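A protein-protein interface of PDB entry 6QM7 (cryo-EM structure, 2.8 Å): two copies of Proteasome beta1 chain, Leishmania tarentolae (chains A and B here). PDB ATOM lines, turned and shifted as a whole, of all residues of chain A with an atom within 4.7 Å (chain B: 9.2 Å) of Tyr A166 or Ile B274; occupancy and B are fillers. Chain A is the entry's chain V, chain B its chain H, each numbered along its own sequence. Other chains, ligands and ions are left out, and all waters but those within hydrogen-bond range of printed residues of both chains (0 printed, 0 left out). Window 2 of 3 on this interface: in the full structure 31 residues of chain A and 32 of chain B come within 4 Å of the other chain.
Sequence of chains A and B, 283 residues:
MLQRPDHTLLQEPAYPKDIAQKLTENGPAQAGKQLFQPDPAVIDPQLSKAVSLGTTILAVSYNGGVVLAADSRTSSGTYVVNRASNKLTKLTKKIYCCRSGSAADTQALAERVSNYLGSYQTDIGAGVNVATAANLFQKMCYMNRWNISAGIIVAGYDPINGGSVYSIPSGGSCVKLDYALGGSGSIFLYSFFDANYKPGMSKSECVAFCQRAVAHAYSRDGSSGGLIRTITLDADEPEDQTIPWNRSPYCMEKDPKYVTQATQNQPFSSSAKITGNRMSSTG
The side-chain amide nitrogen (NE2) of Gln B264 is in hydrogen-bond range of the backbone carbonyl oxygen (O) of Cys A174, 2.8 Å away.
The side-chain amide oxygen (OE1) of Gln B264 lies within hydrogen-bond range of the backbone NH (N) of Lys A176, at 2.9 Å.
O of Ala B272 lies within hydrogen-bond range of ND2 of Asn A161, 3.2 Å away.
The backbone NH (N) of Ile B274 lies within hydrogen-bond range of the side-chain amide oxygen (OD1) of Asn A161.
O of Ala B262 lies within hydrogen-bond range of ND2 of Asn B277, at 2.9 Å.
N of Gln B264 sits at hydrogen-bond distance from OD1 of Asn B277, at 3.0 Å.
OG of Ser B271 lies close to N of Lys B273 (3.3 Å).
The backbone carbonyl oxygen (O) of Val A154 lies within hydrogen-bond range of the backbone NH (N) of Tyr A166 (2.7 Å).
O of Val A175 lies within hydrogen-bond range of N of Ser A167.
Among the printed residues, merely in contact across the chains: Asn A161 with Lys B273 (3.3 Å), Tyr A166 with Ile B274 (3.9 Å), Val A175 with Gln B264 (3.4 Å) and Lys A176 with Ala B262 (3.4 Å).
No residue of chain B comes within 4 Å of Val A154.
No residue of chain B comes within 4 Å of Val A165.
Tyr A166 touches just one residue of chain B: Ile B274.
No residue of chain B comes within 4 Å of Ser A167.
Printed residues of chain B within 4 Å of Val A175: Gln B264.
Of the printed residues of chain A, Ala B262 touches Lys A176 (3.4 Å).
Printed residues of chain A within 4 Å of Lys B273: Asn A161.
Ile B274 touches just these residues of chain A: Asn A161 (2.7 Å) and Tyr A166 (3.9 Å).
The nearest residue of chain B that does not touch Tyr A166 is Gln B264 (5.8 Å).
Hydrophobic or aromatic side chains of chain A within 4 Å of the printed part of chain B: Tyr A166.
Hydrophobic or aromatic side chains of chain B within 4 Å of the printed part of chain A: Ala B262 and Ile B274.
No position is printed for both chains.
Of the 8 pairs that touch across the chains among the printed residues, none has its exchanged pair printed and touching as well.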
ATOM      1  N   VAL A 130     -13.844  -2.495 -23.053  1.00  0.00           N
ATOM      2  CA  VAL A 130     -13.384  -3.041 -24.357  1.00  0.00           C
ATOM      3  C   VAL A 130     -14.609  -3.439 -25.173  1.00  0.00           C
ATOM      4  O   VAL A 130     -14.577  -3.282 -26.406  1.00  0.00           O
ATOM      5  CB  VAL A 130     -12.424  -4.225 -24.179  1.00  0.00           C
ATOM      6  CG1 VAL A 130     -11.981  -4.792 -25.520  1.00  0.00           C
ATOM      7  CG2 VAL A 130     -11.199  -3.822 -23.377  1.00  0.00           C
ATOM      8  N   ALA A 131     -15.638  -3.959 -24.509  1.00  0.00           N
ATOM      9  CA  ALA A 131     -16.920  -4.347 -25.133  1.00  0.00           C
ATOM     10  C   ALA A 131     -17.490  -3.162 -25.911  1.00  0.00           C
ATOM     11  O   ALA A 131     -18.026  -3.389 -27.008  1.00  0.00           O
ATOM     12  CB  ALA A 131     -17.889  -4.816 -24.080  1.00  0.00           C
ATOM     13  N   ALA A 134     -15.445  -2.546 -29.048  1.00  0.00           N
ATOM     14  CA  ALA A 134     -15.701  -3.649 -30.000  1.00  0.00           C
ATOM     15  C   ALA A 134     -17.060  -3.441 -30.654  1.00  0.00           C
ATOM     16  O   ALA A 134     -17.167  -3.606 -31.873  1.00  0.00           O
ATOM     17  CB  ALA A 134     -15.655  -4.978 -29.306  1.00  0.00           C
ATOM     18  N   ILE A 152     -10.683  -6.538 -38.414  1.00  0.00           N
ATOM     19  CA  ILE A 152     -10.294  -5.818 -37.173  1.00  0.00           C
ATOM     20  C   ILE A 152     -10.208  -6.825 -36.034  1.00  0.00           C
ATOM     21  O   ILE A 152     -10.945  -7.808 -36.052  1.00  0.00           O
ATOM     22  CB  ILE A 152     -11.303  -4.691 -36.883  1.00  0.00           C
ATOM     23  CG1 ILE A 152     -11.292  -3.634 -37.987  1.00  0.00           C
ATOM     24  CG2 ILE A 152     -11.065  -4.043 -35.523  1.00  0.00           C
ATOM     25  CD1 ILE A 152      -9.966  -2.894 -38.109  1.00  0.00           C
ATOM     26  N   ILE A 153      -9.286  -6.591 -35.111  1.00  0.00           N
ATOM     27  CA  ILE A 153      -9.253  -7.240 -33.779  1.00  0.00           C
ATOM     28  C   ILE A 153      -9.194  -6.102 -32.784  1.00  0.00           C
ATOM     29  O   ILE A 153      -8.165  -5.446 -32.776  1.00  0.00           O
ATOM     30  CB  ILE A 153      -8.025  -8.146 -33.601  1.00  0.00           C
ATOM     31  CG1 ILE A 153      -8.012  -9.282 -34.614  1.00  0.00           C
ATOM     32  CG2 ILE A 153      -7.955  -8.658 -32.167  1.00  0.00           C
ATOM     33  CD1 ILE A 153      -6.813 -10.152 -34.509  1.00  0.00           C
ATOM     34  N   VAL A 154     -10.248  -5.875 -32.017  1.00  0.00           N
ATOM     35  CA  VAL A 154     -10.254  -4.919 -30.879  1.00  0.00           C
ATOM     36  C   VAL A 154      -9.812  -5.709 -29.672  1.00  0.00           C
ATOM     37  O   VAL A 154     -10.369  -6.770 -29.457  1.00  0.00           O
ATOM     38  CB  VAL A 154     -11.642  -4.321 -30.645  1.00  0.00           C
ATOM     39  CG1 VAL A 154     -11.659  -3.409 -29.434  1.00  0.00           C
ATOM     40  CG2 VAL A 154     -12.129  -3.590 -31.882  1.00  0.00           C
ATOM     41  N   ASN A 161     -13.953  -6.057 -16.830  1.00  0.00           N
ATOM     42  CA  ASN A 161     -13.828  -7.373 -17.509  1.00  0.00           C
ATOM     43  C   ASN A 161     -12.373  -7.795 -17.722  1.00  0.00           C
ATOM     44  O   ASN A 161     -12.171  -8.848 -18.361  1.00  0.00           O
ATOM     45  CB  ASN A 161     -14.545  -7.351 -18.853  1.00  0.00           C
ATOM     46  CG  ASN A 161     -16.014  -7.064 -18.675  1.00  0.00           C
ATOM     47  OD1 ASN A 161     -16.694  -7.785 -17.953  1.00  0.00           O
ATOM     48  ND2 ASN A 161     -16.494  -6.006 -19.305  1.00  0.00           N
ATOM     49  N   SER A 164      -9.655  -8.320 -22.709  1.00  0.00           N
ATOM     50  CA  SER A 164     -10.684  -8.846 -23.629  1.00  0.00           C
ATOM     51  C   SER A 164     -10.150  -8.761 -25.054  1.00  0.00           C
ATOM     52  O   SER A 164      -9.430  -7.832 -25.349  1.00  0.00           O
ATOM     53  CB  SER A 164     -12.016  -8.108 -23.474  1.00  0.00           C
ATOM     54  OG  SER A 164     -12.367  -7.875 -22.107  1.00  0.00           O
ATOM     55  N   VAL A 165     -10.514  -9.711 -25.892  1.00  0.00           N
ATOM     56  CA  VAL A 165     -10.162  -9.730 -27.334  1.00  0.00           C
ATOM     57  C   VAL A 165     -11.453  -9.910 -28.115  1.00  0.00           C
ATOM     58  O   VAL A 165     -12.178 -10.834 -27.803  1.00  0.00           O
ATOM     59  CB  VAL A 165      -9.191 -10.886 -27.616  1.00  0.00           C
ATOM     60  CG1 VAL A 165      -8.925 -11.074 -29.095  1.00  0.00           C
ATOM     61  CG2 VAL A 165      -7.894 -10.698 -26.864  1.00  0.00           C
ATOM     62  N   TYR A 166     -11.705  -9.092 -29.113  1.00  0.00           N
ATOM     63  CA  TYR A 166     -12.860  -9.253 -30.019  1.00  0.00           C
ATOM     64  C   TYR A 166     -12.323  -9.349 -31.444  1.00  0.00           C
ATOM     65  O   TYR A 166     -11.643  -8.439 -31.861  1.00  0.00           O
ATOM     66  CB  TYR A 166     -13.825  -8.076 -29.842  1.00  0.00           C
ATOM     67  CG  TYR A 166     -14.498  -8.007 -28.495  1.00  0.00           C
ATOM     68  CD1 TYR A 166     -15.776  -8.498 -28.303  1.00  0.00           C
ATOM     69  CD2 TYR A 166     -13.852  -7.458 -27.398  1.00  0.00           C
ATOM     70  CE1 TYR A 166     -16.395  -8.443 -27.061  1.00  0.00           C
ATOM     71  CE2 TYR A 166     -14.449  -7.412 -26.145  1.00  0.00           C
ATOM     72  CZ  TYR A 166     -15.727  -7.901 -25.974  1.00  0.00           C
ATOM     73  OH  TYR A 166     -16.306  -7.841 -24.734  1.00  0.00           O
ATOM     74  N   SER A 167     -12.571 -10.432 -32.151  1.00  0.00           N
ATOM     75  CA  SER A 167     -12.388 -10.465 -33.614  1.00  0.00           C
ATOM     76  C   SER A 167     -13.607  -9.802 -34.235  1.00  0.00           C
ATOM     77  O   SER A 167     -14.685 -10.212 -33.877  1.00  0.00           O
ATOM     78  CB  SER A 167     -12.193 -11.875 -34.122  1.00  0.00           C
ATOM     79  OG  SER A 167     -11.675 -11.879 -35.457  1.00  0.00           O
ATOM     80  N   ILE A 168     -13.432  -8.784 -35.071  1.00  0.00           N
ATOM     81  CA  ILE A 168     -14.499  -8.258 -35.967  1.00  0.00           C
ATOM     82  C   ILE A 168     -14.068  -8.526 -37.405  1.00  0.00           C
ATOM     83  O   ILE A 168     -13.495  -7.657 -38.054  1.00  0.00           O
ATOM     84  CB  ILE A 168     -14.781  -6.772 -35.673  1.00  0.00           C
ATOM     85  CG1 ILE A 168     -15.305  -6.583 -34.249  1.00  0.00           C
ATOM     86  CG2 ILE A 168     -15.757  -6.161 -36.668  1.00  0.00           C
ATOM     87  CD1 ILE A 168     -14.627  -5.469 -33.504  1.00  0.00           C
ATOM     88  N   CYS A 174     -18.935  -9.900 -34.535  1.00  0.00           N
ATOM     89  CA  CYS A 174     -18.076  -9.538 -33.381  1.00  0.00           C
ATOM     90  C   CYS A 174     -18.065 -10.720 -32.418  1.00  0.00           C
ATOM     91  O   CYS A 174     -19.118 -10.996 -31.808  1.00  0.00           O
ATOM     92  CB  CYS A 174     -18.589  -8.280 -32.700  1.00  0.00           C
ATOM     93  SG  CYS A 174     -17.555  -7.766 -31.314  1.00  0.00           S
ATOM     94  N   VAL A 175     -16.938 -11.414 -32.332  1.00  0.00           N
ATOM     95  CA  VAL A 175     -16.784 -12.614 -31.474  1.00  0.00           C
ATOM     96  C   VAL A 175     -15.770 -12.279 -30.397  1.00  0.00           C
ATOM     97  O   VAL A 175     -14.705 -11.807 -30.751  1.00  0.00           O
ATOM     98  CB  VAL A 175     -16.342 -13.828 -32.293  1.00  0.00           C
ATOM     99  CG1 VAL A 175     -16.265 -15.075 -31.430  1.00  0.00           C
ATOM    100  CG2 VAL A 175     -17.252 -14.046 -33.487  1.00  0.00           C
ATOM    101  N   LYS A 176     -16.124 -12.506 -29.136  1.00  0.00           N
ATOM    102  CA  LYS A 176     -15.234 -12.326 -27.971  1.00  0.00           C
ATOM    103  C   LYS A 176     -14.493 -13.637 -27.762  1.00  0.00           C
ATOM    104  O   LYS A 176     -15.136 -14.671 -27.689  1.00  0.00           O
ATOM    105  CB  LYS A 176     -16.042 -11.959 -26.733  1.00  0.00           C
ATOM    106  CG  LYS A 176     -15.220 -11.568 -25.517  1.00  0.00           C
ATOM    107  CD  LYS A 176     -16.055 -11.414 -24.267  1.00  0.00           C
ATOM    108  CE  LYS A 176     -15.270 -10.800 -23.130  1.00  0.00           C
ATOM    109  NZ  LYS A 176     -14.034 -11.565 -22.851  1.00  0.00           N
ATOM    110  N   GLN B 261     -16.965 -21.736 -23.982  1.00  0.00           N
ATOM    111  CA  GLN B 261     -17.592 -21.109 -25.163  1.00  0.00           C
ATOM    112  C   GLN B 261     -17.318 -19.609 -25.126  1.00  0.00           C
ATOM    113  O   GLN B 261     -17.266 -19.026 -24.017  1.00  0.00           O
ATOM    114  CB  GLN B 261     -19.093 -21.387 -25.206  1.00  0.00           C
ATOM    115  CG  GLN B 261     -19.437 -22.851 -25.447  1.00  0.00           C
ATOM    116  CD  GLN B 261     -20.810 -23.021 -26.048  1.00  0.00           C
ATOM    117  OE1 GLN B 261     -21.815 -22.681 -25.432  1.00  0.00           O
ATOM    118  NE2 GLN B 261     -20.859 -23.544 -27.262  1.00  0.00           N
ATOM    119  N   ALA B 262     -17.141 -19.019 -26.306  1.00  0.00           N
ATOM    120  CA  ALA B 262     -17.192 -17.562 -26.535  1.00  0.00           C
ATOM    121  C   ALA B 262     -18.421 -17.005 -25.826  1.00  0.00           C
ATOM    122  O   ALA B 262     -19.493 -17.616 -25.931  1.00  0.00           O
ATOM    123  CB  ALA B 262     -17.268 -17.269 -28.007  1.00  0.00           C
ATOM    124  N   THR B 263     -18.268 -15.887 -25.131  1.00  0.00           N
ATOM    125  CA  THR B 263     -19.377 -15.235 -24.406  1.00  0.00           C
ATOM    126  C   THR B 263     -20.085 -14.304 -25.385  1.00  0.00           C
ATOM    127  O   THR B 263     -19.869 -13.093 -25.326  1.00  0.00           O
ATOM    128  CB  THR B 263     -18.858 -14.560 -23.143  1.00  0.00           C
ATOM    129  OG1 THR B 263     -18.197 -15.553 -22.357  1.00  0.00           O
ATOM    130  CG2 THR B 263     -19.990 -13.938 -22.362  1.00  0.00           C
ATOM    131  N   GLN B 264     -20.871 -14.888 -26.277  1.00  0.00           N
ATOM    132  CA  GLN B 264     -21.542 -14.194 -27.398  1.00  0.00           C
ATOM    133  C   GLN B 264     -22.963 -13.820 -27.016  1.00  0.00           C
ATOM    134  O   GLN B 264     -23.454 -12.815 -27.559  1.00  0.00           O
ATOM    135  CB  GLN B 264     -21.618 -15.095 -28.630  1.00  0.00           C
ATOM    136  CG  GLN B 264     -20.293 -15.256 -29.350  1.00  0.00           C
ATOM    137  CD  GLN B 264     -19.719 -13.908 -29.700  1.00  0.00           C
ATOM    138  OE1 GLN B 264     -18.920 -13.355 -28.954  1.00  0.00           O
ATOM    139  NE2 GLN B 264     -20.177 -13.344 -30.805  1.00  0.00           N
ATOM    140  N   ASN B 265     -23.616 -14.617 -26.174  1.00  0.00           N
ATOM    141  CA  ASN B 265     -25.088 -14.551 -26.007  1.00  0.00           C
ATOM    142  C   ASN B 265     -25.383 -13.532 -24.917  1.00  0.00           C
ATOM    143  O   ASN B 265     -25.798 -12.414 -25.289  1.00  0.00           O
ATOM    144  CB  ASN B 265     -25.687 -15.947 -25.883  1.00  0.00           C
ATOM    145  CG  ASN B 265     -25.637 -16.674 -27.216  1.00  0.00           C
ATOM    146  OD1 ASN B 265     -25.562 -16.052 -28.272  1.00  0.00           O
ATOM    147  ND2 ASN B 265     -25.664 -17.994 -27.180  1.00  0.00           N
ATOM    148  N   GLN B 266     -25.106 -13.847 -23.659  1.00  0.00           N
ATOM    149  CA  GLN B 266     -24.990 -12.830 -22.572  1.00  0.00           C
ATOM    150  C   GLN B 266     -26.364 -12.354 -22.119  1.00  0.00           C
ATOM    151  O   GLN B 266     -27.105 -11.732 -22.876  1.00  0.00           O
ATOM    152  CB  GLN B 266     -24.179 -11.603 -22.989  1.00  0.00           C
ATOM    153  CG  GLN B 266     -23.328 -11.034 -21.860  1.00  0.00           C
ATOM    154  CD  GLN B 266     -22.285 -10.113 -22.447  1.00  0.00           C
ATOM    155  OE1 GLN B 266     -22.313  -8.898 -22.245  1.00  0.00           O
ATOM    156  NE2 GLN B 266     -21.383 -10.688 -23.234  1.00  0.00           N
ATOM    157  N   PRO B 267     -26.729 -12.606 -20.847  1.00  0.00           N
ATOM    158  CA  PRO B 267     -28.055 -12.252 -20.368  1.00  0.00           C
ATOM    159  C   PRO B 267     -28.150 -10.731 -20.269  1.00  0.00           C
ATOM    160  O   PRO B 267     -27.130 -10.064 -20.125  1.00  0.00           O
ATOM    161  CB  PRO B 267     -28.180 -12.955 -19.006  1.00  0.00           C
ATOM    162  CG  PRO B 267     -26.746 -13.161 -18.548  1.00  0.00           C
ATOM    163  CD  PRO B 267     -25.897 -13.217 -19.800  1.00  0.00           C
ATOM    164  N   SER B 269     -28.491  -7.619 -18.474  1.00  0.00           N
ATOM    165  CA  SER B 269     -27.963  -7.339 -17.118  1.00  0.00           C
ATOM    166  C   SER B 269     -27.963  -5.840 -16.862  1.00  0.00           C
ATOM    167  O   SER B 269     -28.146  -5.077 -17.790  1.00  0.00           O
ATOM    168  CB  SER B 269     -26.592  -7.906 -16.921  1.00  0.00           C
ATOM    169  OG  SER B 269     -25.619  -7.048 -17.479  1.00  0.00           O
ATOM    170  N   SER B 271     -25.364  -4.405 -15.542  1.00  0.00           N
ATOM    171  CA  SER B 271     -23.899  -4.258 -15.400  1.00  0.00           C
ATOM    172  C   SER B 271     -23.238  -4.522 -16.756  1.00  0.00           C
ATOM    173  O   SER B 271     -23.804  -5.264 -17.567  1.00  0.00           O
ATOM    174  CB  SER B 271     -23.387  -5.196 -14.334  1.00  0.00           C
ATOM    175  OG  SER B 271     -22.007  -4.972 -14.063  1.00  0.00           O
ATOM    176  N   ALA B 272     -22.075  -3.920 -16.986  1.00  0.00           N
ATOM    177  CA  ALA B 272     -21.231  -4.133 -18.183  1.00  0.00           C
ATOM    178  C   ALA B 272     -20.310  -5.326 -17.947  1.00  0.00           C
ATOM    179  O   ALA B 272     -19.604  -5.697 -18.895  1.00  0.00           O
ATOM    180  CB  ALA B 272     -20.438  -2.886 -18.497  1.00  0.00           C
ATOM    181  N   LYS B 273     -20.314  -5.887 -16.737  1.00  0.00           N
ATOM    182  CA  LYS B 273     -19.552  -7.110 -16.399  1.00  0.00           C
ATOM    183  C   LYS B 273     -20.072  -8.280 -17.239  1.00  0.00           C
ATOM    184  O   LYS B 273     -21.220  -8.696 -17.022  1.00  0.00           O
ATOM    185  CB  LYS B 273     -19.659  -7.431 -14.910  1.00  0.00           C
ATOM    186  CG  LYS B 273     -18.892  -8.681 -14.507  1.00  0.00           C
ATOM    187  CD  LYS B 273     -18.244  -8.614 -13.135  1.00  0.00           C
ATOM    188  CE  LYS B 273     -16.791  -9.048 -13.149  1.00  0.00           C
ATOM    189  NZ  LYS B 273     -16.606 -10.355 -13.828  1.00  0.00           N
ATOM    190  N   ILE B 274     -19.252  -8.768 -18.171  1.00  0.00           N
ATOM    191  CA  ILE B 274     -19.478 -10.038 -18.920  1.00  0.00           C
ATOM    192  C   ILE B 274     -19.322 -11.191 -17.926  1.00  0.00           C
ATOM    193  O   ILE B 274     -18.224 -11.334 -17.364  1.00  0.00           O
ATOM    194  CB  ILE B 274     -18.522 -10.170 -20.127  1.00  0.00           C
ATOM    195  CG1 ILE B 274     -18.965  -9.315 -21.322  1.00  0.00           C
ATOM    196  CG2 ILE B 274     -18.357 -11.624 -20.531  1.00  0.00           C
ATOM    197  CD1 ILE B 274     -18.344  -7.937 -21.390  1.00  0.00           C
ATOM    198  N   THR B 275     -20.394 -11.964 -17.730  1.00  0.00           N
ATOM    199  CA  THR B 275     -20.468 -13.160 -16.846  1.00  0.00           C
ATOM    200  C   THR B 275     -20.251 -14.418 -17.698  1.00  0.00           C
ATOM    201  O   THR B 275     -19.133 -14.971 -17.662  1.00  0.00           O
ATOM    202  CB  THR B 275     -21.807 -13.184 -16.096  1.00  0.00           C
ATOM    203  OG1 THR B 275     -22.844 -12.990 -17.062  1.00  0.00           O
ATOM    204  CG2 THR B 275     -21.894 -12.124 -15.018  1.00  0.00           C
ATOM    205  N   GLY B 276     -21.275 -14.836 -18.443  1.00  0.00           N
ATOM    206  CA  GLY B 276     -21.230 -16.016 -19.323  1.00  0.00           C
ATOM    207  C   GLY B 276     -22.337 -15.955 -20.354  1.00  0.00           C
ATOM    208  O   GLY B 276     -22.979 -14.903 -20.456  1.00  0.00           O
ATOM    209  N   ASN B 277     -22.549 -17.035 -21.100  1.00  0.00           N
ATOM    210  CA  ASN B 277     -23.708 -17.154 -22.013  1.00  0.00           C
ATOM    211  C   ASN B 277     -24.969 -17.428 -21.195  1.00  0.00           C
ATOM    212  O   ASN B 277     -24.885 -18.139 -20.185  1.00  0.00           O
ATOM    213  CB  ASN B 277     -23.515 -18.237 -23.066  1.00  0.00           C
ATOM    214  CG  ASN B 277     -22.420 -17.873 -24.033  1.00  0.00           C
ATOM    215  OD1 ASN B 277     -22.495 -16.843 -24.687  1.00  0.00           O
ATOM    216  ND2 ASN B 277     -21.405 -18.714 -24.120  1.00  0.00           N
